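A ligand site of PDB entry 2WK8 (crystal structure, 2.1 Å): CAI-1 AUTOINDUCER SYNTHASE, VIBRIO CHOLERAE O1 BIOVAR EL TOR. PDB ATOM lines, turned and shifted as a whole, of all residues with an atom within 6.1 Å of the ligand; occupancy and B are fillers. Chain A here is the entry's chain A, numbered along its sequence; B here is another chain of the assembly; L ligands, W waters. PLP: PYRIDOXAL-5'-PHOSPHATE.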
ATOM      1  N   ASN A  47     -15.023 -15.981 -17.029  1.00  0.00           N
ATOM      2  CA  ASN A  47     -15.608 -17.251 -16.616  1.00  0.00           C
ATOM      3  C   ASN A  47     -14.672 -18.383 -16.980  1.00  0.00           C
ATOM      4  O   ASN A  47     -15.044 -19.555 -16.897  1.00  0.00           O
ATOM      5  CB  ASN A  47     -16.937 -17.446 -17.333  1.00  0.00           C
ATOM      6  CG  ASN A  47     -17.932 -16.355 -16.999  1.00  0.00           C
ATOM      7  OD1 ASN A  47     -18.261 -15.512 -17.840  1.00  0.00           O
ATOM      8  ND2 ASN A  47     -18.418 -16.361 -15.775  1.00  0.00           N
ATOM      9  N   GLN A 106     -25.388 -23.390 -30.136  1.00  0.00           N
ATOM     10  CA  GLN A 106     -24.517 -22.259 -30.483  1.00  0.00           C
ATOM     11  C   GLN A 106     -24.126 -21.441 -29.255  1.00  0.00           C
ATOM     12  O   GLN A 106     -23.244 -20.594 -29.321  1.00  0.00           O
ATOM     13  CB  GLN A 106     -25.117 -21.381 -31.592  1.00  0.00           C
ATOM     14  CG  GLN A 106     -25.605 -22.173 -32.812  1.00  0.00           C
ATOM     15  CD  GLN A 106     -27.101 -22.449 -32.748  1.00  0.00           C
ATOM     16  OE1 GLN A 106     -27.638 -22.711 -31.678  1.00  0.00           O
ATOM     17  NE2 GLN A 106     -27.771 -22.389 -33.905  1.00  0.00           N
ATOM     18  N   SER A 107     -24.762 -21.723 -28.126  1.00  0.00           N
ATOM     19  CA  SER A 107     -24.477 -20.993 -26.898  1.00  0.00           C
ATOM     20  C   SER A 107     -25.201 -21.719 -25.806  1.00  0.00           C
ATOM     21  O   SER A 107     -26.089 -22.524 -26.089  1.00  0.00           O
ATOM     22  CB  SER A 107     -25.006 -19.558 -27.002  1.00  0.00           C
ATOM     23  OG  SER A 107     -26.418 -19.534 -27.193  1.00  0.00           O
ATOM     24  N   GLY A 108     -24.846 -21.442 -24.549  1.00  0.00           N
ATOM     25  CA  GLY A 108     -25.585 -21.931 -23.410  1.00  0.00           C
ATOM     26  C   GLY A 108     -27.011 -21.408 -23.377  1.00  0.00           C
ATOM     27  O   GLY A 108     -27.940 -22.123 -22.968  1.00  0.00           O
ATOM     28  N   TRP A 109     -27.199 -20.156 -23.799  1.00  0.00           N
ATOM     29  CA  TRP A 109     -28.525 -19.555 -23.874  1.00  0.00           C
ATOM     30  C   TRP A 109     -29.395 -20.411 -24.811  1.00  0.00           C
ATOM     31  O   TRP A 109     -30.501 -20.795 -24.462  1.00  0.00           O
ATOM     32  CB  TRP A 109     -28.449 -18.100 -24.396  1.00  0.00           C
ATOM     33  CG  TRP A 109     -29.800 -17.405 -24.514  1.00  0.00           C
ATOM     34  CD1 TRP A 109     -30.700 -17.525 -25.530  1.00  0.00           C
ATOM     35  CD2 TRP A 109     -30.369 -16.481 -23.580  1.00  0.00           C
ATOM     36  NE1 TRP A 109     -31.801 -16.734 -25.296  1.00  0.00           N
ATOM     37  CE2 TRP A 109     -31.630 -16.084 -24.097  1.00  0.00           C
ATOM     38  CE3 TRP A 109     -29.954 -15.945 -22.350  1.00  0.00           C
ATOM     39  CZ2 TRP A 109     -32.477 -15.192 -23.426  1.00  0.00           C
ATOM     40  CZ3 TRP A 109     -30.792 -15.050 -21.681  1.00  0.00           C
ATOM     41  CH2 TRP A 109     -32.040 -14.687 -22.221  1.00  0.00           C
ATOM     42  N   ASN A 110     -28.877 -20.707 -25.997  1.00  0.00           N
ATOM     43  CA  ASN A 110     -29.619 -21.497 -26.957  1.00  0.00           C
ATOM     44  C   ASN A 110     -29.913 -22.904 -26.446  1.00  0.00           C
ATOM     45  O   ASN A 110     -30.991 -23.432 -26.684  1.00  0.00           O
ATOM     46  CB  ASN A 110     -28.923 -21.534 -28.325  1.00  0.00           C
ATOM     47  CG  ASN A 110     -29.038 -20.205 -29.071  1.00  0.00           C
ATOM     48  OD1 ASN A 110     -29.581 -19.234 -28.523  1.00  0.00           O
ATOM     49  ND2 ASN A 110     -28.522 -20.158 -30.312  1.00  0.00           N
ATOM     50  N   ASN A 112     -30.480 -23.875 -23.440  1.00  0.00           N
ATOM     51  CA  ASN A 112     -31.603 -23.793 -22.514  1.00  0.00           C
ATOM     52  C   ASN A 112     -32.952 -23.473 -23.202  1.00  0.00           C
ATOM     53  O   ASN A 112     -33.982 -24.091 -22.913  1.00  0.00           O
ATOM     54  CB  ASN A 112     -31.300 -22.782 -21.405  1.00  0.00           C
ATOM     55  CG  ASN A 112     -30.360 -23.314 -20.342  1.00  0.00           C
ATOM     56  OD1 ASN A 112     -30.191 -24.544 -20.175  1.00  0.00           O
ATOM     57  ND2 ASN A 112     -29.742 -22.409 -19.610  1.00  0.00           N
ATOM     58  N   HIS A 133     -30.808 -19.056 -14.131  1.00  0.00           N
ATOM     59  CA  HIS A 133     -30.339 -18.130 -15.164  1.00  0.00           C
ATOM     60  C   HIS A 133     -31.467 -17.575 -16.039  1.00  0.00           C
ATOM     61  O   HIS A 133     -32.468 -18.246 -16.291  1.00  0.00           O
ATOM     62  CB  HIS A 133     -29.272 -18.795 -16.034  1.00  0.00           C
ATOM     63  CG  HIS A 133     -28.556 -17.837 -16.923  1.00  0.00           C
ATOM     64  ND1 HIS A 133     -28.813 -17.736 -18.270  1.00  0.00           N
ATOM     65  CD2 HIS A 133     -27.598 -16.915 -16.646  1.00  0.00           C
ATOM     66  CE1 HIS A 133     -28.029 -16.804 -18.799  1.00  0.00           C
ATOM     67  NE2 HIS A 133     -27.283 -16.300 -17.834  1.00  0.00           N
ATOM     68  N   SER A 135     -31.748 -17.313 -19.173  1.00  0.00           N
ATOM     69  CA  SER A 135     -32.048 -18.164 -20.324  1.00  0.00           C
ATOM     70  C   SER A 135     -33.100 -19.213 -19.978  1.00  0.00           C
ATOM     71  O   SER A 135     -33.846 -19.683 -20.849  1.00  0.00           O
ATOM     72  CB  SER A 135     -30.778 -18.864 -20.847  1.00  0.00           C
ATOM     73  OG  SER A 135     -30.160 -19.641 -19.820  1.00  0.00           O
ATOM     74  N   LEU A 136     -33.121 -19.612 -18.712  1.00  0.00           N
ATOM     75  CA  LEU A 136     -34.055 -20.636 -18.259  1.00  0.00           C
ATOM     76  C   LEU A 136     -35.430 -20.002 -18.048  1.00  0.00           C
ATOM     77  O   LEU A 136     -36.444 -20.591 -18.402  1.00  0.00           O
ATOM     78  CB  LEU A 136     -33.568 -21.315 -16.985  1.00  0.00           C
ATOM     79  CG  LEU A 136     -32.367 -22.235 -17.202  1.00  0.00           C
ATOM     80  CD1 LEU A 136     -31.612 -22.452 -15.905  1.00  0.00           C
ATOM     81  CD2 LEU A 136     -32.809 -23.559 -17.792  1.00  0.00           C
ATOM     82  N   ASP A 173     -29.843 -23.993 -11.571  1.00  0.00           N
ATOM     83  CA  ASP A 173     -28.413 -23.915 -11.812  1.00  0.00           C
ATOM     84  C   ASP A 173     -27.746 -24.826 -10.769  1.00  0.00           C
ATOM     85  O   ASP A 173     -28.122 -24.802  -9.594  1.00  0.00           O
ATOM     86  CB  ASP A 173     -27.892 -22.492 -11.542  1.00  0.00           C
ATOM     87  CG  ASP A 173     -28.343 -21.442 -12.564  1.00  0.00           C
ATOM     88  OD1 ASP A 173     -29.281 -21.677 -13.391  1.00  0.00           O
ATOM     89  OD2 ASP A 173     -27.759 -20.335 -12.512  1.00  0.00           O
ATOM     90  N   ILE A 175     -24.544 -24.340  -9.891  1.00  0.00           N
ATOM     91  CA  ILE A 175     -23.904 -23.245  -9.186  1.00  0.00           C
ATOM     92  C   ILE A 175     -24.439 -21.949  -9.772  1.00  0.00           C
ATOM     93  O   ILE A 175     -24.466 -21.732 -10.980  1.00  0.00           O
ATOM     94  CB  ILE A 175     -22.371 -23.310  -9.288  1.00  0.00           C
ATOM     95  CG1 ILE A 175     -21.853 -24.578  -8.596  1.00  0.00           C
ATOM     96  CG2 ILE A 175     -21.743 -22.065  -8.667  1.00  0.00           C
ATOM     97  CD1 ILE A 175     -20.350 -24.849  -8.800  1.00  0.00           C
ATOM     98  N   SER A 177     -25.048 -18.213 -10.959  1.00  0.00           N
ATOM     99  CA  SER A 177     -24.096 -17.393 -11.705  1.00  0.00           C
ATOM    100  C   SER A 177     -23.797 -16.058 -11.037  1.00  0.00           C
ATOM    101  O   SER A 177     -22.710 -15.506 -11.188  1.00  0.00           O
ATOM    102  CB  SER A 177     -24.541 -17.219 -13.169  1.00  0.00           C
ATOM    103  OG  SER A 177     -25.844 -16.704 -13.263  1.00  0.00           O
ATOM    104  N   ASP A 202     -28.575 -26.838 -14.887  1.00  0.00           N
ATOM    105  CA  ASP A 202     -27.634 -26.050 -15.672  1.00  0.00           C
ATOM    106  C   ASP A 202     -26.274 -26.019 -14.954  1.00  0.00           C
ATOM    107  O   ASP A 202     -26.092 -25.302 -13.972  1.00  0.00           O
ATOM    108  CB  ASP A 202     -28.188 -24.645 -15.894  1.00  0.00           C
ATOM    109  CG  ASP A 202     -27.305 -23.803 -16.778  1.00  0.00           C
ATOM    110  OD1 ASP A 202     -26.079 -24.036 -16.814  1.00  0.00           O
ATOM    111  OD2 ASP A 202     -27.834 -22.874 -17.434  1.00  0.00           O
ATOM    112  N   SER A 204     -23.402 -24.791 -15.974  1.00  0.00           N
ATOM    113  CA  SER A 204     -22.475 -23.863 -16.633  1.00  0.00           C
ATOM    114  C   SER A 204     -21.272 -23.466 -15.769  1.00  0.00           C
ATOM    115  O   SER A 204     -20.154 -23.252 -16.284  1.00  0.00           O
ATOM    116  CB  SER A 204     -23.219 -22.618 -17.110  1.00  0.00           C
ATOM    117  OG  SER A 204     -24.138 -22.925 -18.142  1.00  0.00           O
ATOM    118  N   HIS A 205     -21.495 -23.358 -14.458  1.00  0.00           N
ATOM    119  CA  HIS A 205     -20.434 -22.933 -13.544  1.00  0.00           C
ATOM    120  C   HIS A 205     -19.789 -24.051 -12.733  1.00  0.00           C
ATOM    121  O   HIS A 205     -18.945 -23.785 -11.876  1.00  0.00           O
ATOM    122  CB  HIS A 205     -20.931 -21.790 -12.672  1.00  0.00           C
ATOM    123  CG  HIS A 205     -21.379 -20.614 -13.480  1.00  0.00           C
ATOM    124  ND1 HIS A 205     -20.497 -19.672 -13.965  1.00  0.00           N
ATOM    125  CD2 HIS A 205     -22.602 -20.261 -13.943  1.00  0.00           C
ATOM    126  CE1 HIS A 205     -21.163 -18.771 -14.661  1.00  0.00           C
ATOM    127  NE2 HIS A 205     -22.433 -19.102 -14.663  1.00  0.00           N
ATOM    128  N   THR A 231     -27.615 -29.105 -18.856  1.00  0.00           N
ATOM    129  CA  THR A 231     -27.148 -28.153 -19.870  1.00  0.00           C
ATOM    130  C   THR A 231     -25.931 -27.374 -19.393  1.00  0.00           C
ATOM    131  O   THR A 231     -25.650 -27.309 -18.198  1.00  0.00           O
ATOM    132  CB  THR A 231     -28.213 -27.116 -20.225  1.00  0.00           C
ATOM    133  OG1 THR A 231     -28.486 -26.337 -19.058  1.00  0.00           O
ATOM    134  CG2 THR A 231     -29.517 -27.800 -20.741  1.00  0.00           C
ATOM    135  N   ALA A 232     -25.208 -26.770 -20.327  1.00  0.00           N
ATOM    136  CA  ALA A 232     -24.093 -25.922 -19.947  1.00  0.00           C
ATOM    137  C   ALA A 232     -23.703 -25.007 -21.081  1.00  0.00           C
ATOM    138  O   ALA A 232     -23.732 -25.393 -22.251  1.00  0.00           O
ATOM    139  CB  ALA A 232     -22.885 -26.766 -19.508  1.00  0.00           C
ATOM    140  N   SER A 233     -23.338 -23.777 -20.733  1.00  0.00           N
ATOM    141  CA  SER A 233     -22.593 -22.937 -21.639  1.00  0.00           C
ATOM    142  C   SER A 233     -21.224 -23.593 -21.674  1.00  0.00           C
ATOM    143  O   SER A 233     -20.747 -24.071 -20.650  1.00  0.00           O
ATOM    144  CB  SER A 233     -22.460 -21.524 -21.061  1.00  0.00           C
ATOM    145  OG  SER A 233     -21.528 -20.759 -21.807  1.00  0.00           O
ATOM    146  N   LEU A 234     -20.575 -23.573 -22.835  1.00  0.00           N
ATOM    147  CA  LEU A 234     -19.224 -24.103 -22.948  1.00  0.00           C
ATOM    148  C   LEU A 234     -18.281 -22.921 -22.947  1.00  0.00           C
ATOM    149  O   LEU A 234     -17.072 -23.078 -23.170  1.00  0.00           O
ATOM    150  CB  LEU A 234     -19.079 -24.870 -24.242  1.00  0.00           C
ATOM    151  CG  LEU A 234     -19.174 -26.392 -24.307  1.00  0.00           C
ATOM    152  CD1 LEU A 234     -19.674 -27.089 -23.035  1.00  0.00           C
ATOM    153  CD2 LEU A 234     -19.943 -26.791 -25.524  1.00  0.00           C
ATOM    154  N   ALA A 235     -18.850 -21.749 -22.688  1.00  0.00           N
ATOM    155  CA  ALA A 235     -18.135 -20.483 -22.718  1.00  0.00           C
ATOM    156  C   ALA A 235     -17.596 -20.090 -21.343  1.00  0.00           C
ATOM    157  O   ALA A 235     -17.218 -18.951 -21.139  1.00  0.00           O
ATOM    158  CB  ALA A 235     -19.020 -19.366 -23.251  1.00  0.00           C
ATOM    159  N   LYS A 236     -17.582 -21.044 -20.418  1.00  0.00           N
ATOM    160  CA  LYS A 236     -17.022 -20.819 -19.104  1.00  0.00           C
ATOM    161  C   LYS A 236     -15.712 -21.587 -19.008  1.00  0.00           C
ATOM    162  O   LYS A 236     -14.712 -21.198 -19.596  1.00  0.00           O
ATOM    163  CB  LYS A 236     -17.995 -21.278 -18.031  1.00  0.00           C
ATOM    164  CG  LYS A 236     -19.435 -20.839 -18.284  1.00  0.00           C
ATOM    165  CD  LYS A 236     -19.556 -19.307 -18.315  1.00  0.00           C
ATOM    166  CE  LYS A 236     -21.017 -18.895 -18.485  1.00  0.00           C
ATOM    167  NZ  LYS A 236     -21.178 -17.430 -18.696  1.00  0.00           N
ATOM    168  N   TYR A 240     -15.189 -21.438 -24.669  1.00  0.00           N
ATOM    169  CA  TYR A 240     -15.599 -21.394 -26.071  1.00  0.00           C
ATOM    170  C   TYR A 240     -17.053 -20.986 -26.265  1.00  0.00           C
ATOM    171  O   TYR A 240     -17.925 -21.283 -25.436  1.00  0.00           O
ATOM    172  CB  TYR A 240     -15.379 -22.741 -26.744  1.00  0.00           C
ATOM    173  CG  TYR A 240     -15.266 -22.598 -28.237  1.00  0.00           C
ATOM    174  CD1 TYR A 240     -14.147 -22.008 -28.809  1.00  0.00           C
ATOM    175  CD2 TYR A 240     -16.298 -23.009 -29.080  1.00  0.00           C
ATOM    176  CE1 TYR A 240     -14.035 -21.859 -30.185  1.00  0.00           C
ATOM    177  CE2 TYR A 240     -16.194 -22.872 -30.457  1.00  0.00           C
ATOM    178  CZ  TYR A 240     -15.067 -22.299 -31.003  1.00  0.00           C
ATOM    179  OH  TYR A 240     -14.951 -22.155 -32.360  1.00  0.00           O
ATOM    180  N   ARG A 241     -17.317 -20.304 -27.377  1.00  0.00           N
ATOM    181  CA  ARG A 241     -18.629 -19.737 -27.645  1.00  0.00           C
ATOM    182  C   ARG A 241     -19.584 -20.781 -28.211  1.00  0.00           C
ATOM    183  O   ARG A 241     -19.794 -20.845 -29.412  1.00  0.00           O
ATOM    184  CB  ARG A 241     -18.505 -18.554 -28.602  1.00  0.00           C
ATOM    185  CG  ARG A 241     -19.784 -17.740 -28.768  1.00  0.00           C
ATOM    186  CD  ARG A 241     -19.523 -16.458 -29.539  1.00  0.00           C
ATOM    187  NE  ARG A 241     -18.950 -16.727 -30.857  1.00  0.00           N
ATOM    188  CZ  ARG A 241     -19.658 -16.802 -31.969  1.00  0.00           C
ATOM    189  NH1 ARG A 241     -20.974 -16.611 -31.903  1.00  0.00           N
ATOM    190  NH2 ARG A 241     -19.067 -17.038 -33.145  1.00  0.00           N
ATOM    191  N   ALA A 242     -20.167 -21.571 -27.328  1.00  0.00           N
ATOM    192  CA  ALA A 242     -21.059 -22.663 -27.709  1.00  0.00           C
ATOM    193  C   ALA A 242     -21.811 -23.077 -26.441  1.00  0.00           C
ATOM    194  O   ALA A 242     -21.659 -22.461 -25.384  1.00  0.00           O
ATOM    195  CB  ALA A 242     -20.263 -23.847 -28.277  1.00  0.00           C
ATOM    196  N   GLY A 243     -22.630 -24.116 -26.580  1.00  0.00           N
ATOM    197  CA  GLY A 243     -23.367 -24.693 -25.466  1.00  0.00           C
ATOM    198  C   GLY A 243     -23.683 -26.141 -25.768  1.00  0.00           C
ATOM    199  O   GLY A 243     -23.404 -26.613 -26.863  1.00  0.00           O
ATOM    200  N   ARG A 358     -19.809  -9.096  -8.921  1.00  0.00           N
ATOM    201  CA  ARG A 358     -19.332 -10.462  -8.861  1.00  0.00           C
ATOM    202  C   ARG A 358     -17.822 -10.587  -8.985  1.00  0.00           C
ATOM    203  O   ARG A 358     -17.230 -10.054  -9.919  1.00  0.00           O
ATOM    204  CB  ARG A 358     -20.003 -11.308  -9.948  1.00  0.00           C
ATOM    205  CG  ARG A 358     -19.537 -12.755  -9.972  1.00  0.00           C
ATOM    206  CD  ARG A 358     -20.303 -13.562 -11.025  1.00  0.00           C
ATOM    207  NE  ARG A 358     -19.847 -13.246 -12.380  1.00  0.00           N
ATOM    208  CZ  ARG A 358     -20.386 -13.774 -13.484  1.00  0.00           C
ATOM    209  NH1 ARG A 358     -21.391 -14.630 -13.372  1.00  0.00           N
ATOM    210  NH2 ARG A 358     -19.915 -13.441 -14.679  1.00  0.00           N
ATOM    211  N   PHE B 264     -26.834 -11.656 -21.710  1.00  0.00           N
ATOM    212  CA  PHE B 264     -26.686 -12.901 -20.980  1.00  0.00           C
ATOM    213  C   PHE B 264     -26.060 -14.021 -21.800  1.00  0.00           C
ATOM    214  O   PHE B 264     -26.099 -15.182 -21.397  1.00  0.00           O
ATOM    215  CB  PHE B 264     -28.044 -13.411 -20.501  1.00  0.00           C
ATOM    216  CG  PHE B 264     -28.787 -12.426 -19.670  1.00  0.00           C
ATOM    217  CD1 PHE B 264     -28.442 -12.246 -18.341  1.00  0.00           C
ATOM    218  CD2 PHE B 264     -29.825 -11.690 -20.199  1.00  0.00           C
ATOM    219  CE1 PHE B 264     -29.127 -11.335 -17.554  1.00  0.00           C
ATOM    220  CE2 PHE B 264     -30.513 -10.777 -19.421  1.00  0.00           C
ATOM    221  CZ  PHE B 264     -30.158 -10.595 -18.093  1.00  0.00           C
ATOM    222  N   SER B 265     -25.514 -13.676 -22.966  1.00  0.00           N
ATOM    223  CA  SER B 265     -24.841 -14.665 -23.782  1.00  0.00           C
ATOM    224  C   SER B 265     -23.472 -14.156 -24.146  1.00  0.00           C
ATOM    225  O   SER B 265     -23.322 -13.002 -24.513  1.00  0.00           O
ATOM    226  CB  SER B 265     -25.658 -14.989 -25.021  1.00  0.00           C
ATOM    227  OG  SER B 265     -25.368 -16.266 -25.511  1.00  0.00           O
ATOM    228  N   SER B 266     -22.465 -15.035 -24.064  1.00  0.00           N
ATOM    229  CA  SER B 266     -21.089 -14.616 -24.306  1.00  0.00           C
ATOM    230  C   SER B 266     -20.882 -13.998 -25.691  1.00  0.00           C
ATOM    231  O   SER B 266     -21.501 -14.397 -26.699  1.00  0.00           O
ATOM    232  CB  SER B 266     -20.094 -15.767 -24.061  1.00  0.00           C
ATOM    233  OG  SER B 266     -19.994 -16.632 -25.191  1.00  0.00           O
ATOM    234  N   THR B 267     -19.986 -13.018 -25.703  1.00  0.00           N
ATOM    235  CA  THR B 267     -19.592 -12.268 -26.882  1.00  0.00           C
ATOM    236  C   THR B 267     -18.713 -13.087 -27.816  1.00  0.00           C
ATOM    237  O   THR B 267     -18.152 -14.100 -27.424  1.00  0.00           O
ATOM    238  CB  THR B 267     -18.794 -11.036 -26.420  1.00  0.00           C
ATOM    239  OG1 THR B 267     -18.443 -10.225 -27.542  1.00  0.00           O
ATOM    240  CG2 THR B 267     -17.533 -11.462 -25.699  1.00  0.00           C
HETATM  241  N1  PLP L   1     -26.601 -20.693 -17.989  1.00  0.00           N
HETATM  242  C2  PLP L   1     -25.979 -20.053 -16.938  1.00  0.00           C
HETATM  243  C2A PLP L   1     -26.161 -20.559 -15.527  1.00  0.00           C
HETATM  244  C3  PLP L   1     -25.216 -18.915 -17.183  1.00  0.00           C
HETATM  245  O3  PLP L   1     -24.593 -18.263 -16.171  1.00  0.00           O
HETATM  246  C4  PLP L   1     -25.038 -18.435 -18.472  1.00  0.00           C
HETATM  247  C4A PLP L   1     -24.281 -17.147 -18.591  1.00  0.00           C
HETATM  248  O4A PLP L   1     -23.621 -16.870 -19.589  1.00  0.00           O
HETATM  249  C5  PLP L   1     -25.669 -19.093 -19.538  1.00  0.00           C
HETATM  250  C6  PLP L   1     -26.441 -20.226 -19.278  1.00  0.00           C
HETATM  251  C5A PLP L   1     -25.543 -18.640 -20.971  1.00  0.00           C
HETATM  252  O4P PLP L   1     -24.355 -19.140 -21.569  1.00  0.00           O
HETATM  253  P   PLP L   1     -23.863 -18.612 -23.013  1.00  0.00           P
HETATM  254  O1P PLP L   1     -23.092 -17.347 -22.843  1.00  0.00           O
HETATM  255  O2P PLP L   1     -25.077 -18.347 -23.874  1.00  0.00           O
HETATM  256  O3P PLP L   1     -22.992 -19.680 -23.620  1.00  0.00           O
HETATM  257  O   HOH W   1     -21.778 -15.515 -20.860  1.00  0.00           O
HETATM  258  O   HOH W   2     -21.746 -18.963 -25.799  1.00  0.00           O
HETATM  259  O   HOH W   3     -25.198 -14.546 -17.884  1.00  0.00           O
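OD1 of Asp 202 lies within hydrogen-bond range of OG of Ser 204, 2.6 Å away. The side-chain carboxylate (OD2) of Asp 202 is in hydrogen-bond range of the side-chain amide nitrogen (ND2) of Asn 112 (2.9 Å). The backbone NH (N) of Ser 233 lies within hydrogen-bond range of the side-chain hydroxyl (OG) of Ser 204 (2.8 Å). The backbone NH (N) of Gly 108 sits at hydrogen-bond distance from the backbone carbonyl oxygen (O) of Ala 242 (3.4 Å). The backbone NH (N) of His 133 sits at hydrogen-bond distance from the side-chain carboxylate (OD1) of Asp 173, at 3.1 Å. The backbone carbonyl oxygen (O) of Ala 242 lies within hydrogen-bond range of the backbone NH (N) of Leu 234, 3.0 Å away. The side-chain hydroxyl (OG) of Ser 135 is in hydrogen-bond range of the side-chain amide nitrogen (ND2) of Asn 112, at 2.8 Å. The side-chain amide oxygen of Asn 112 sits at hydrogen-bond distance from the side-chain hydroxyl of Thr 231 (2.7 Å).
CB of Ser 107 touches O2P of the ligand, 3.4 Å away. ND2 of Asn 112 touches N1 of the ligand, at 3.9 Å. His 133 touches the ligand. Ser 135 touches the ligand. OD2 of Asp 173 touches C2A of the ligand, 3.4 Å away. CB of Ser 177 touches O3 of the ligand (3.2 Å). Ala 242 touches the ligand (O to O3P, 3.6 Å). Phe 264 of chain B touches the ligand. Hydrophobic or aromatic side chains within 4 Å of the ligand: Trp 109, His 133 and His 205. Of the 31 residues printed, 17 come within 4 Å of the ligand.
The side-chain carboxylate of Asp 202 sits at hydrogen-bond distance from a nitrogen (N1) of the ligand (2.6 Å). An oxygen (O3P) of the ligand lies within hydrogen-bond range of the side-chain hydroxyl (OG) of Ser 233, at 2.6 Å. The side-chain amino group (NZ) of Lys 236 sits at hydrogen-bond distance from an oxygen (O4A) of the ligand. An oxygen (O2P) of the ligand lies within hydrogen-bond range of the side-chain hydroxyl (OG) of Ser 265 of chain B (2.7 Å). O1P of the ligand lies within hydrogen-bond range of N of Ser 266 of chain B (2.7 Å). N of Gly 108 is in hydrogen-bond range of O3P of the ligand, at 2.7 Å. A ring nitrogen (NE2) of His 205 is in hydrogen-bond range of an oxygen (O3) of the ligand (2.8 Å). The backbone NH (N) of Trp 109 lies within hydrogen-bond range of an oxygen (O2P) of the ligand (2.8 Å). The side-chain hydroxyl (OG) of Ser 204 sits at hydrogen-bond distance from a nitrogen (N1) of the ligand.
Water W2 lies within hydrogen-bond range of an oxygen (O3P) of the ligand, the side-chain hydroxyl (OG) of Ser 266 of chain B and the backbone NH (N) of Ala 242. Water W1 lies within hydrogen-bond range of O4A of the ligand (2.6 Å), NZ of Lys 236 (3.0 Å) and N of Ser 266 of chain B (3.3 Å). Water W3 lies within hydrogen-bond range of a ring nitrogen (NE2) of His 133 and an oxygen (O4A) of the ligand.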
